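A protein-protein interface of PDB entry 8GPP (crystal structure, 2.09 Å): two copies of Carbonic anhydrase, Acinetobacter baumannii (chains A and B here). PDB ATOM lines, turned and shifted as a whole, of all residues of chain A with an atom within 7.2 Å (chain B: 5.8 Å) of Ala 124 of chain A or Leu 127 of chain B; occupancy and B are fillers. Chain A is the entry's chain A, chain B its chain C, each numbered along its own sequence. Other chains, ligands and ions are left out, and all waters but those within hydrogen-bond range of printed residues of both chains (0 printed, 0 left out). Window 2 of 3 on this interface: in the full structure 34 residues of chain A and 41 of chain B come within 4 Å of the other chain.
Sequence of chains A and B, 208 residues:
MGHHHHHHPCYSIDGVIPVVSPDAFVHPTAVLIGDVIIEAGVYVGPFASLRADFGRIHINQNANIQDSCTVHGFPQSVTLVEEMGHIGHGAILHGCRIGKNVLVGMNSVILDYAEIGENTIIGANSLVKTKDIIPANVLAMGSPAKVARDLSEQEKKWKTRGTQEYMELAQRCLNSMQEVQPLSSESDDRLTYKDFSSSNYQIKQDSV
Hydrophobic or aromatic side chains of chain A that line the printed part of chain B: Met 106 and Ala 124.
Among the printed residues, no Asp or Glu carboxylate lies within 4 Å of a Lys or Arg side-chain nitrogen of the other chain.
Ala 124 of chain A touches just one residue of chain B: Leu 127.
Of the printed residues of chain A, Leu 127 of chain B touches Ala 124 and Asn 125.
Printed residues of chain B within 4 Å of Asn 125 of chain A: Val 109, Asn 125, Ser 126, Leu 127 and Ser 143.
Printed residues of chain A within 4 Å of Val 109 of chain B: Met 106, Asn 107 and Asn 125.
Printed residues of chain A within 4 Å of Leu 111 of chain B: Met 106 (3.5 Å).
The nearest residue of chain B that does not touch Ala 124 of chain A is Val 109 of chain B (4.6 Å).
Among the printed residues, pairs that only touch across the chains: Met 106 of chain A with Val 109 of chain B, Met 106 of chain A with Leu 111 of chain B, Asn 107 of chain A with Val 109 of chain B, Ala 124 of chain A with Leu 127 of chain B, Asn 125 of chain A with Val 109 of chain B, Asn 125 of chain A with Asn 125 of chain B, Asn 125 of chain A with Ser 126 of chain B, Asn 125 of chain A with Leu 127 of chain B and Asn 125 of chain A with Ser 143 of chain B.
Asn 125 of chain B touches its own counterpart, Asn 125 of chain A.
Asn 125 of chain A touches Ser 126 of chain B, but with the chains exchanged Ser 126 of chain A does not touch Asn 125 of chain B (9.0 Å).
Asn 125 of chain A touches Leu 127 of chain B, but with the chains exchanged Leu 127 of chain A does not touch Asn 125 of chain B (9.7 Å).
Of the 9 pairs that touch across the chains among the printed residues, 1 has its exchanged pair printed and touching as well.
N of Asn 125 of chain A sits at hydrogen-bond distance from OG of Ser 108 of chain A.
O of Ala 124 of chain A is in hydrogen-bond range of OG of Ser 126 of chain A (3.5 Å).
N of Ser 126 of chain B lies within hydrogen-bond range of OG of Ser 108 of chain B.
The backbone NH (N) of Val 109 of chain B is in hydrogen-bond range of the backbone carbonyl oxygen (O) of Ser 126 of chain B, 2.8 Å away.
N of Val 128 of chain B sits at hydrogen-bond distance from O of Val 109 of chain B, 2.8 Å away.
The backbone NH (N) of Leu 111 of chain B sits at hydrogen-bond distance from the backbone carbonyl oxygen (O) of Val 128 of chain B (3.1 Å).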
ATOM      1  N   VAL A 104     -25.474 -26.463   2.134  1.00  0.00           N
ATOM      2  CA  VAL A 104     -24.933 -25.544   1.136  1.00  0.00           C
ATOM      3  C   VAL A 104     -24.862 -26.319  -0.166  1.00  0.00           C
ATOM      4  O   VAL A 104     -24.051 -27.248  -0.300  1.00  0.00           O
ATOM      5  CB  VAL A 104     -23.557 -25.008   1.542  1.00  0.00           C
ATOM      6  CG1 VAL A 104     -22.980 -24.120   0.437  1.00  0.00           C
ATOM      7  CG2 VAL A 104     -23.672 -24.232   2.835  1.00  0.00           C
ATOM      8  N   GLY A 105     -25.739 -25.978  -1.109  1.00  0.00           N
ATOM      9  CA  GLY A 105     -25.820 -26.742  -2.339  1.00  0.00           C
ATOM     10  C   GLY A 105     -24.512 -26.741  -3.109  1.00  0.00           C
ATOM     11  O   GLY A 105     -23.685 -25.832  -3.006  1.00  0.00           O
ATOM     12  N   MET A 106     -24.339 -27.778  -3.926  1.00  0.00           N
ATOM     13  CA  MET A 106     -23.081 -27.961  -4.639  1.00  0.00           C
ATOM     14  C   MET A 106     -22.764 -26.777  -5.538  1.00  0.00           C
ATOM     15  O   MET A 106     -23.657 -26.097  -6.066  1.00  0.00           O
ATOM     16  CB  MET A 106     -23.087 -29.272  -5.442  1.00  0.00           C
ATOM     17  CG  MET A 106     -24.378 -29.657  -6.121  1.00  0.00           C
ATOM     18  SD  MET A 106     -24.332 -31.436  -6.501  1.00  0.00           S
ATOM     19  CE  MET A 106     -25.678 -32.070  -5.455  1.00  0.00           C
ATOM     20  N   ASN A 107     -21.463 -26.507  -5.665  1.00  0.00           N
ATOM     21  CA  ASN A 107     -20.928 -25.469  -6.547  1.00  0.00           C
ATOM     22  C   ASN A 107     -21.354 -24.062  -6.112  1.00  0.00           C
ATOM     23  O   ASN A 107     -21.345 -23.130  -6.915  1.00  0.00           O
ATOM     24  CB  ASN A 107     -21.344 -25.729  -8.004  1.00  0.00           C
ATOM     25  CG  ASN A 107     -20.298 -25.280  -9.008  1.00  0.00           C
ATOM     26  OD1 ASN A 107     -19.109 -25.192  -8.696  1.00  0.00           O
ATOM     27  ND2 ASN A 107     -20.733 -25.023 -10.239  1.00  0.00           N
ATOM     28  N   SER A 108     -21.721 -23.877  -4.855  1.00  0.00           N
ATOM     29  CA  SER A 108     -22.156 -22.576  -4.357  1.00  0.00           C
ATOM     30  C   SER A 108     -21.000 -21.828  -3.714  1.00  0.00           C
ATOM     31  O   SER A 108     -20.011 -22.423  -3.269  1.00  0.00           O
ATOM     32  CB  SER A 108     -23.281 -22.730  -3.336  1.00  0.00           C
ATOM     33  OG  SER A 108     -24.476 -23.181  -3.965  1.00  0.00           O
ATOM     34  N   ILE A 121     -31.592 -24.230   3.571  1.00  0.00           N
ATOM     35  CA  ILE A 121     -31.028 -24.944   2.431  1.00  0.00           C
ATOM     36  C   ILE A 121     -30.631 -23.918   1.364  1.00  0.00           C
ATOM     37  O   ILE A 121     -31.463 -23.127   0.905  1.00  0.00           O
ATOM     38  CB  ILE A 121     -32.012 -25.985   1.869  1.00  0.00           C
ATOM     39  CG1 ILE A 121     -32.206 -27.138   2.870  1.00  0.00           C
ATOM     40  CG2 ILE A 121     -31.511 -26.530   0.540  1.00  0.00           C
ATOM     41  CD1 ILE A 121     -33.063 -28.310   2.336  1.00  0.00           C
ATOM     42  N   ILE A 122     -29.374 -23.948   0.946  1.00  0.00           N
ATOM     43  CA  ILE A 122     -28.901 -23.090  -0.137  1.00  0.00           C
ATOM     44  C   ILE A 122     -28.846 -23.924  -1.402  1.00  0.00           C
ATOM     45  O   ILE A 122     -28.145 -24.941  -1.449  1.00  0.00           O
ATOM     46  CB  ILE A 122     -27.529 -22.483   0.180  1.00  0.00           C
ATOM     47  CG1 ILE A 122     -27.612 -21.667   1.461  1.00  0.00           C
ATOM     48  CG2 ILE A 122     -27.050 -21.602  -0.979  1.00  0.00           C
ATOM     49  CD1 ILE A 122     -28.542 -20.488   1.333  1.00  0.00           C
ATOM     50  N   GLY A 123     -29.569 -23.491  -2.427  1.00  0.00           N
ATOM     51  CA  GLY A 123     -29.594 -24.231  -3.677  1.00  0.00           C
ATOM     52  C   GLY A 123     -28.241 -24.272  -4.363  1.00  0.00           C
ATOM     53  O   GLY A 123     -27.359 -23.438  -4.139  1.00  0.00           O
ATOM     54  N   ALA A 124     -28.086 -25.277  -5.228  1.00  0.00           N
ATOM     55  CA  ALA A 124     -26.842 -25.447  -5.964  1.00  0.00           C
ATOM     56  C   ALA A 124     -26.554 -24.223  -6.825  1.00  0.00           C
ATOM     57  O   ALA A 124     -27.461 -23.538  -7.304  1.00  0.00           O
ATOM     58  CB  ALA A 124     -26.908 -26.702  -6.835  1.00  0.00           C
ATOM     59  N   ASN A 125     -25.267 -23.968  -7.050  1.00  0.00           N
ATOM     60  CA  ASN A 125     -24.821 -22.900  -7.951  1.00  0.00           C
ATOM     61  C   ASN A 125     -25.234 -21.524  -7.451  1.00  0.00           C
ATOM     62  O   ASN A 125     -25.405 -20.594  -8.239  1.00  0.00           O
ATOM     63  CB  ASN A 125     -25.334 -23.112  -9.377  1.00  0.00           C
ATOM     64  CG  ASN A 125     -24.431 -24.021 -10.182  1.00  0.00           C
ATOM     65  OD1 ASN A 125     -23.470 -24.598  -9.647  1.00  0.00           O
ATOM     66  ND2 ASN A 125     -24.739 -24.176 -11.468  1.00  0.00           N
ATOM     67  N   SER A 126     -25.405 -21.377  -6.151  1.00  0.00           N
ATOM     68  CA  SER A 126     -25.860 -20.112  -5.607  1.00  0.00           C
ATOM     69  C   SER A 126     -24.665 -19.289  -5.157  1.00  0.00           C
ATOM     70  O   SER A 126     -23.541 -19.789  -5.057  1.00  0.00           O
ATOM     71  CB  SER A 126     -26.812 -20.336  -4.427  1.00  0.00           C
ATOM     72  OG  SER A 126     -27.887 -21.189  -4.777  1.00  0.00           O
ATOM     73  N   LEU A 127     -24.925 -18.007  -4.888  1.00  0.00           N
ATOM     74  CA  LEU A 127     -23.903 -17.078  -4.419  1.00  0.00           C
ATOM     75  C   LEU A 127     -24.496 -16.228  -3.304  1.00  0.00           C
ATOM     76  O   LEU A 127     -25.451 -15.477  -3.532  1.00  0.00           O
ATOM     77  CB  LEU A 127     -23.385 -16.189  -5.567  1.00  0.00           C
ATOM     78  CG  LEU A 127     -22.532 -14.964  -5.207  1.00  0.00           C
ATOM     79  CD1 LEU A 127     -21.236 -15.391  -4.518  1.00  0.00           C
ATOM     80  CD2 LEU A 127     -22.208 -14.119  -6.434  1.00  0.00           C
ATOM     81  N   LEU A 139     -35.478 -21.817   2.199  1.00  0.00           N
ATOM     82  CA  LEU A 139     -34.759 -22.155   0.983  1.00  0.00           C
ATOM     83  C   LEU A 139     -34.314 -20.862   0.316  1.00  0.00           C
ATOM     84  O   LEU A 139     -35.132 -19.966   0.099  1.00  0.00           O
ATOM     85  CB  LEU A 139     -35.639 -22.962   0.031  1.00  0.00           C
ATOM     86  CG  LEU A 139     -34.948 -23.261  -1.298  1.00  0.00           C
ATOM     87  CD1 LEU A 139     -33.831 -24.283  -1.099  1.00  0.00           C
ATOM     88  CD2 LEU A 139     -35.952 -23.725  -2.348  1.00  0.00           C
ATOM     89  N   ALA A 140     -33.024 -20.755   0.016  1.00  0.00           N
ATOM     90  CA  ALA A 140     -32.497 -19.617  -0.731  1.00  0.00           C
ATOM     91  C   ALA A 140     -31.623 -20.113  -1.876  1.00  0.00           C
ATOM     92  O   ALA A 140     -30.865 -21.083  -1.723  1.00  0.00           O
ATOM     93  CB  ALA A 140     -31.699 -18.653   0.166  1.00  0.00           C
ATOM     94  N   MET A 141     -31.726 -19.444  -3.019  1.00  0.00           N
ATOM     95  CA  MET A 141     -30.969 -19.855  -4.188  1.00  0.00           C
ATOM     96  C   MET A 141     -30.740 -18.656  -5.091  1.00  0.00           C
ATOM     97  O   MET A 141     -31.286 -17.573  -4.880  1.00  0.00           O
ATOM     98  CB  MET A 141     -31.697 -20.946  -4.970  1.00  0.00           C
ATOM     99  CG  MET A 141     -33.055 -20.477  -5.435  1.00  0.00           C
ATOM    100  SD  MET A 141     -34.290 -21.753  -5.208  1.00  0.00           S
ATOM    101  CE  MET A 141     -33.983 -22.758  -6.678  1.00  0.00           C
ATOM    102  N   GLY A 142     -29.937 -18.874  -6.119  1.00  0.00           N
ATOM    103  CA  GLY A 142     -29.669 -17.846  -7.106  1.00  0.00           C
ATOM    104  C   GLY A 142     -28.303 -17.228  -6.934  1.00  0.00           C
ATOM    105  O   GLY A 142     -27.544 -17.524  -6.006  1.00  0.00           O
ATOM    106  N   SER B 108     -20.467 -27.049 -14.649  1.00  0.00           N
ATOM    107  CA  SER B 108     -21.894 -27.329 -14.637  1.00  0.00           C
ATOM    108  C   SER B 108     -22.240 -28.376 -13.579  1.00  0.00           C
ATOM    109  O   SER B 108     -21.401 -29.173 -13.159  1.00  0.00           O
ATOM    110  CB  SER B 108     -22.357 -27.810 -16.007  1.00  0.00           C
ATOM    111  OG  SER B 108     -22.159 -26.816 -17.004  1.00  0.00           O
ATOM    112  N   VAL B 109     -23.508 -28.368 -13.167  1.00  0.00           N
ATOM    113  CA  VAL B 109     -24.056 -29.300 -12.187  1.00  0.00           C
ATOM    114  C   VAL B 109     -25.216 -30.034 -12.851  1.00  0.00           C
ATOM    115  O   VAL B 109     -26.154 -29.395 -13.346  1.00  0.00           O
ATOM    116  CB  VAL B 109     -24.515 -28.578 -10.907  1.00  0.00           C
ATOM    117  CG1 VAL B 109     -25.151 -29.530  -9.947  1.00  0.00           C
ATOM    118  CG2 VAL B 109     -23.338 -27.882 -10.220  1.00  0.00           C
ATOM    119  N   ILE B 110     -25.136 -31.370 -12.885  1.00  0.00           N
ATOM    120  CA  ILE B 110     -26.175 -32.244 -13.453  1.00  0.00           C
ATOM    121  C   ILE B 110     -26.735 -33.101 -12.322  1.00  0.00           C
ATOM    122  O   ILE B 110     -26.066 -34.035 -11.858  1.00  0.00           O
ATOM    123  CB  ILE B 110     -25.633 -33.139 -14.568  1.00  0.00           C
ATOM    124  CG1 ILE B 110     -24.713 -32.343 -15.520  1.00  0.00           C
ATOM    125  CG2 ILE B 110     -26.786 -33.801 -15.319  1.00  0.00           C
ATOM    126  CD1 ILE B 110     -25.415 -31.288 -16.325  1.00  0.00           C
ATOM    127  N   LEU B 111     -27.966 -32.815 -11.898  1.00  0.00           N
ATOM    128  CA  LEU B 111     -28.495 -33.374 -10.657  1.00  0.00           C
ATOM    129  C   LEU B 111     -29.219 -34.707 -10.901  1.00  0.00           C
ATOM    130  O   LEU B 111     -29.205 -35.270 -12.004  1.00  0.00           O
ATOM    131  CB  LEU B 111     -29.397 -32.352  -9.965  1.00  0.00           C
ATOM    132  CG  LEU B 111     -28.622 -31.163  -9.380  1.00  0.00           C
ATOM    133  CD1 LEU B 111     -29.567 -30.146  -8.752  1.00  0.00           C
ATOM    134  CD2 LEU B 111     -27.548 -31.615  -8.387  1.00  0.00           C
ATOM    135  N   ASN B 125     -21.146 -23.548 -16.747  1.00  0.00           N
ATOM    136  CA  ASN B 125     -21.809 -22.908 -15.608  1.00  0.00           C
ATOM    137  C   ASN B 125     -23.302 -23.203 -15.570  1.00  0.00           C
ATOM    138  O   ASN B 125     -24.079 -22.427 -15.002  1.00  0.00           O
ATOM    139  CB  ASN B 125     -21.571 -21.396 -15.612  1.00  0.00           C
ATOM    140  CG  ASN B 125     -20.501 -20.977 -14.616  1.00  0.00           C
ATOM    141  OD1 ASN B 125     -19.635 -21.785 -14.253  1.00  0.00           O
ATOM    142  ND2 ASN B 125     -20.540 -19.709 -14.178  1.00  0.00           N
ATOM    143  N   SER B 126     -23.725 -24.317 -16.164  1.00  0.00           N
ATOM    144  CA  SER B 126     -25.142 -24.643 -16.210  1.00  0.00           C
ATOM    145  C   SER B 126     -25.563 -25.529 -15.028  1.00  0.00           C
ATOM    146  O   SER B 126     -24.747 -26.199 -14.394  1.00  0.00           O
ATOM    147  CB  SER B 126     -25.472 -25.331 -17.529  1.00  0.00           C
ATOM    148  OG  SER B 126     -25.179 -24.461 -18.612  1.00  0.00           O
ATOM    149  N   LEU B 127     -26.859 -25.506 -14.725  1.00  0.00           N
ATOM    150  CA  LEU B 127     -27.442 -26.371 -13.704  1.00  0.00           C
ATOM    151  C   LEU B 127     -28.630 -27.095 -14.316  1.00  0.00           C
ATOM    152  O   LEU B 127     -29.600 -26.455 -14.722  1.00  0.00           O
ATOM    153  CB  LEU B 127     -27.877 -25.579 -12.466  1.00  0.00           C
ATOM    154  CG  LEU B 127     -28.793 -26.355 -11.504  1.00  0.00           C
ATOM    155  CD1 LEU B 127     -28.018 -27.299 -10.592  1.00  0.00           C
ATOM    156  CD2 LEU B 127     -29.650 -25.426 -10.669  1.00  0.00           C
ATOM    157  N   VAL B 128     -28.553 -28.419 -14.402  1.00  0.00           N
ATOM    158  CA  VAL B 128     -29.666 -29.234 -14.889  1.00  0.00           C
ATOM    159  C   VAL B 128     -30.402 -29.805 -13.690  1.00  0.00           C
ATOM    160  O   VAL B 128     -29.844 -30.618 -12.946  1.00  0.00           O
ATOM    161  CB  VAL B 128     -29.188 -30.366 -15.807  1.00  0.00           C
ATOM    162  CG1 VAL B 128     -30.379 -31.270 -16.169  1.00  0.00           C
ATOM    163  CG2 VAL B 128     -28.505 -29.814 -17.046  1.00  0.00           C
ATOM    164  N   LYS B 129     -31.662 -29.412 -13.521  1.00  0.00           N
ATOM    165  CA  LYS B 129     -32.427 -29.746 -12.325  1.00  0.00           C
ATOM    166  C   LYS B 129     -32.713 -31.245 -12.235  1.00  0.00           C
ATOM    167  O   LYS B 129     -32.755 -31.968 -13.237  1.00  0.00           O
ATOM    168  CB  LYS B 129     -33.760 -28.993 -12.301  1.00  0.00           C
ATOM    169  CG  LYS B 129     -33.665 -27.469 -12.177  1.00  0.00           C
ATOM    170  CD  LYS B 129     -32.735 -27.049 -11.042  1.00  0.00           C
ATOM    171  CE  LYS B 129     -33.518 -26.754  -9.768  1.00  0.00           C
ATOM    172  NZ  LYS B 129     -32.591 -26.588  -8.599  1.00  0.00           N
ATOM    173  N   GLY B 142     -27.742 -22.335 -18.872  1.00  0.00           N
ATOM    174  CA  GLY B 142     -28.413 -21.552 -17.859  1.00  0.00           C
ATOM    175  C   GLY B 142     -28.533 -22.312 -16.552  1.00  0.00           C
ATOM    176  O   GLY B 142     -28.234 -23.503 -16.447  1.00  0.00           O
ATOM    177  N   SER B 143     -28.986 -21.579 -15.537  1.00  0.00           N
ATOM    178  CA  SER B 143     -29.019 -22.080 -14.165  1.00  0.00           C
ATOM    179  C   SER B 143     -30.278 -21.539 -13.502  1.00  0.00           C
ATOM    180  O   SER B 143     -30.246 -20.501 -12.828  1.00  0.00           O
ATOM    181  CB  SER B 143     -27.755 -21.667 -13.411  1.00  0.00           C
ATOM    182  OG  SER B 143     -27.791 -22.075 -12.066  1.00  0.00           O
ATOM    183  N   PRO B 144     -31.423 -22.230 -13.669  1.00  0.00           N
ATOM    184  CA  PRO B 144     -31.547 -23.574 -14.251  1.00  0.00           C
ATOM    185  C   PRO B 144     -31.491 -23.618 -15.783  1.00  0.00           C
ATOM    186  O   PRO B 144     -32.036 -22.743 -16.460  1.00  0.00           O
ATOM    187  CB  PRO B 144     -32.920 -24.040 -13.754  1.00  0.00           C
ATOM    188  CG  PRO B 144     -33.680 -22.783 -13.424  1.00  0.00           C
ATOM    189  CD  PRO B 144     -32.740 -21.605 -13.481  1.00  0.00           C
ATOM    190  N   ALA B 145     -30.846 -24.659 -16.309  1.00  0.00           N
ATOM    191  CA  ALA B 145     -30.614 -24.779 -17.740  1.00  0.00           C
ATOM    192  C   ALA B 145     -31.930 -24.808 -18.503  1.00  0.00           C
ATOM    193  O   ALA B 145     -32.990 -25.142 -17.968  1.00  0.00           O
ATOM    194  CB  ALA B 145     -29.814 -26.045 -18.055  1.00  0.00           C
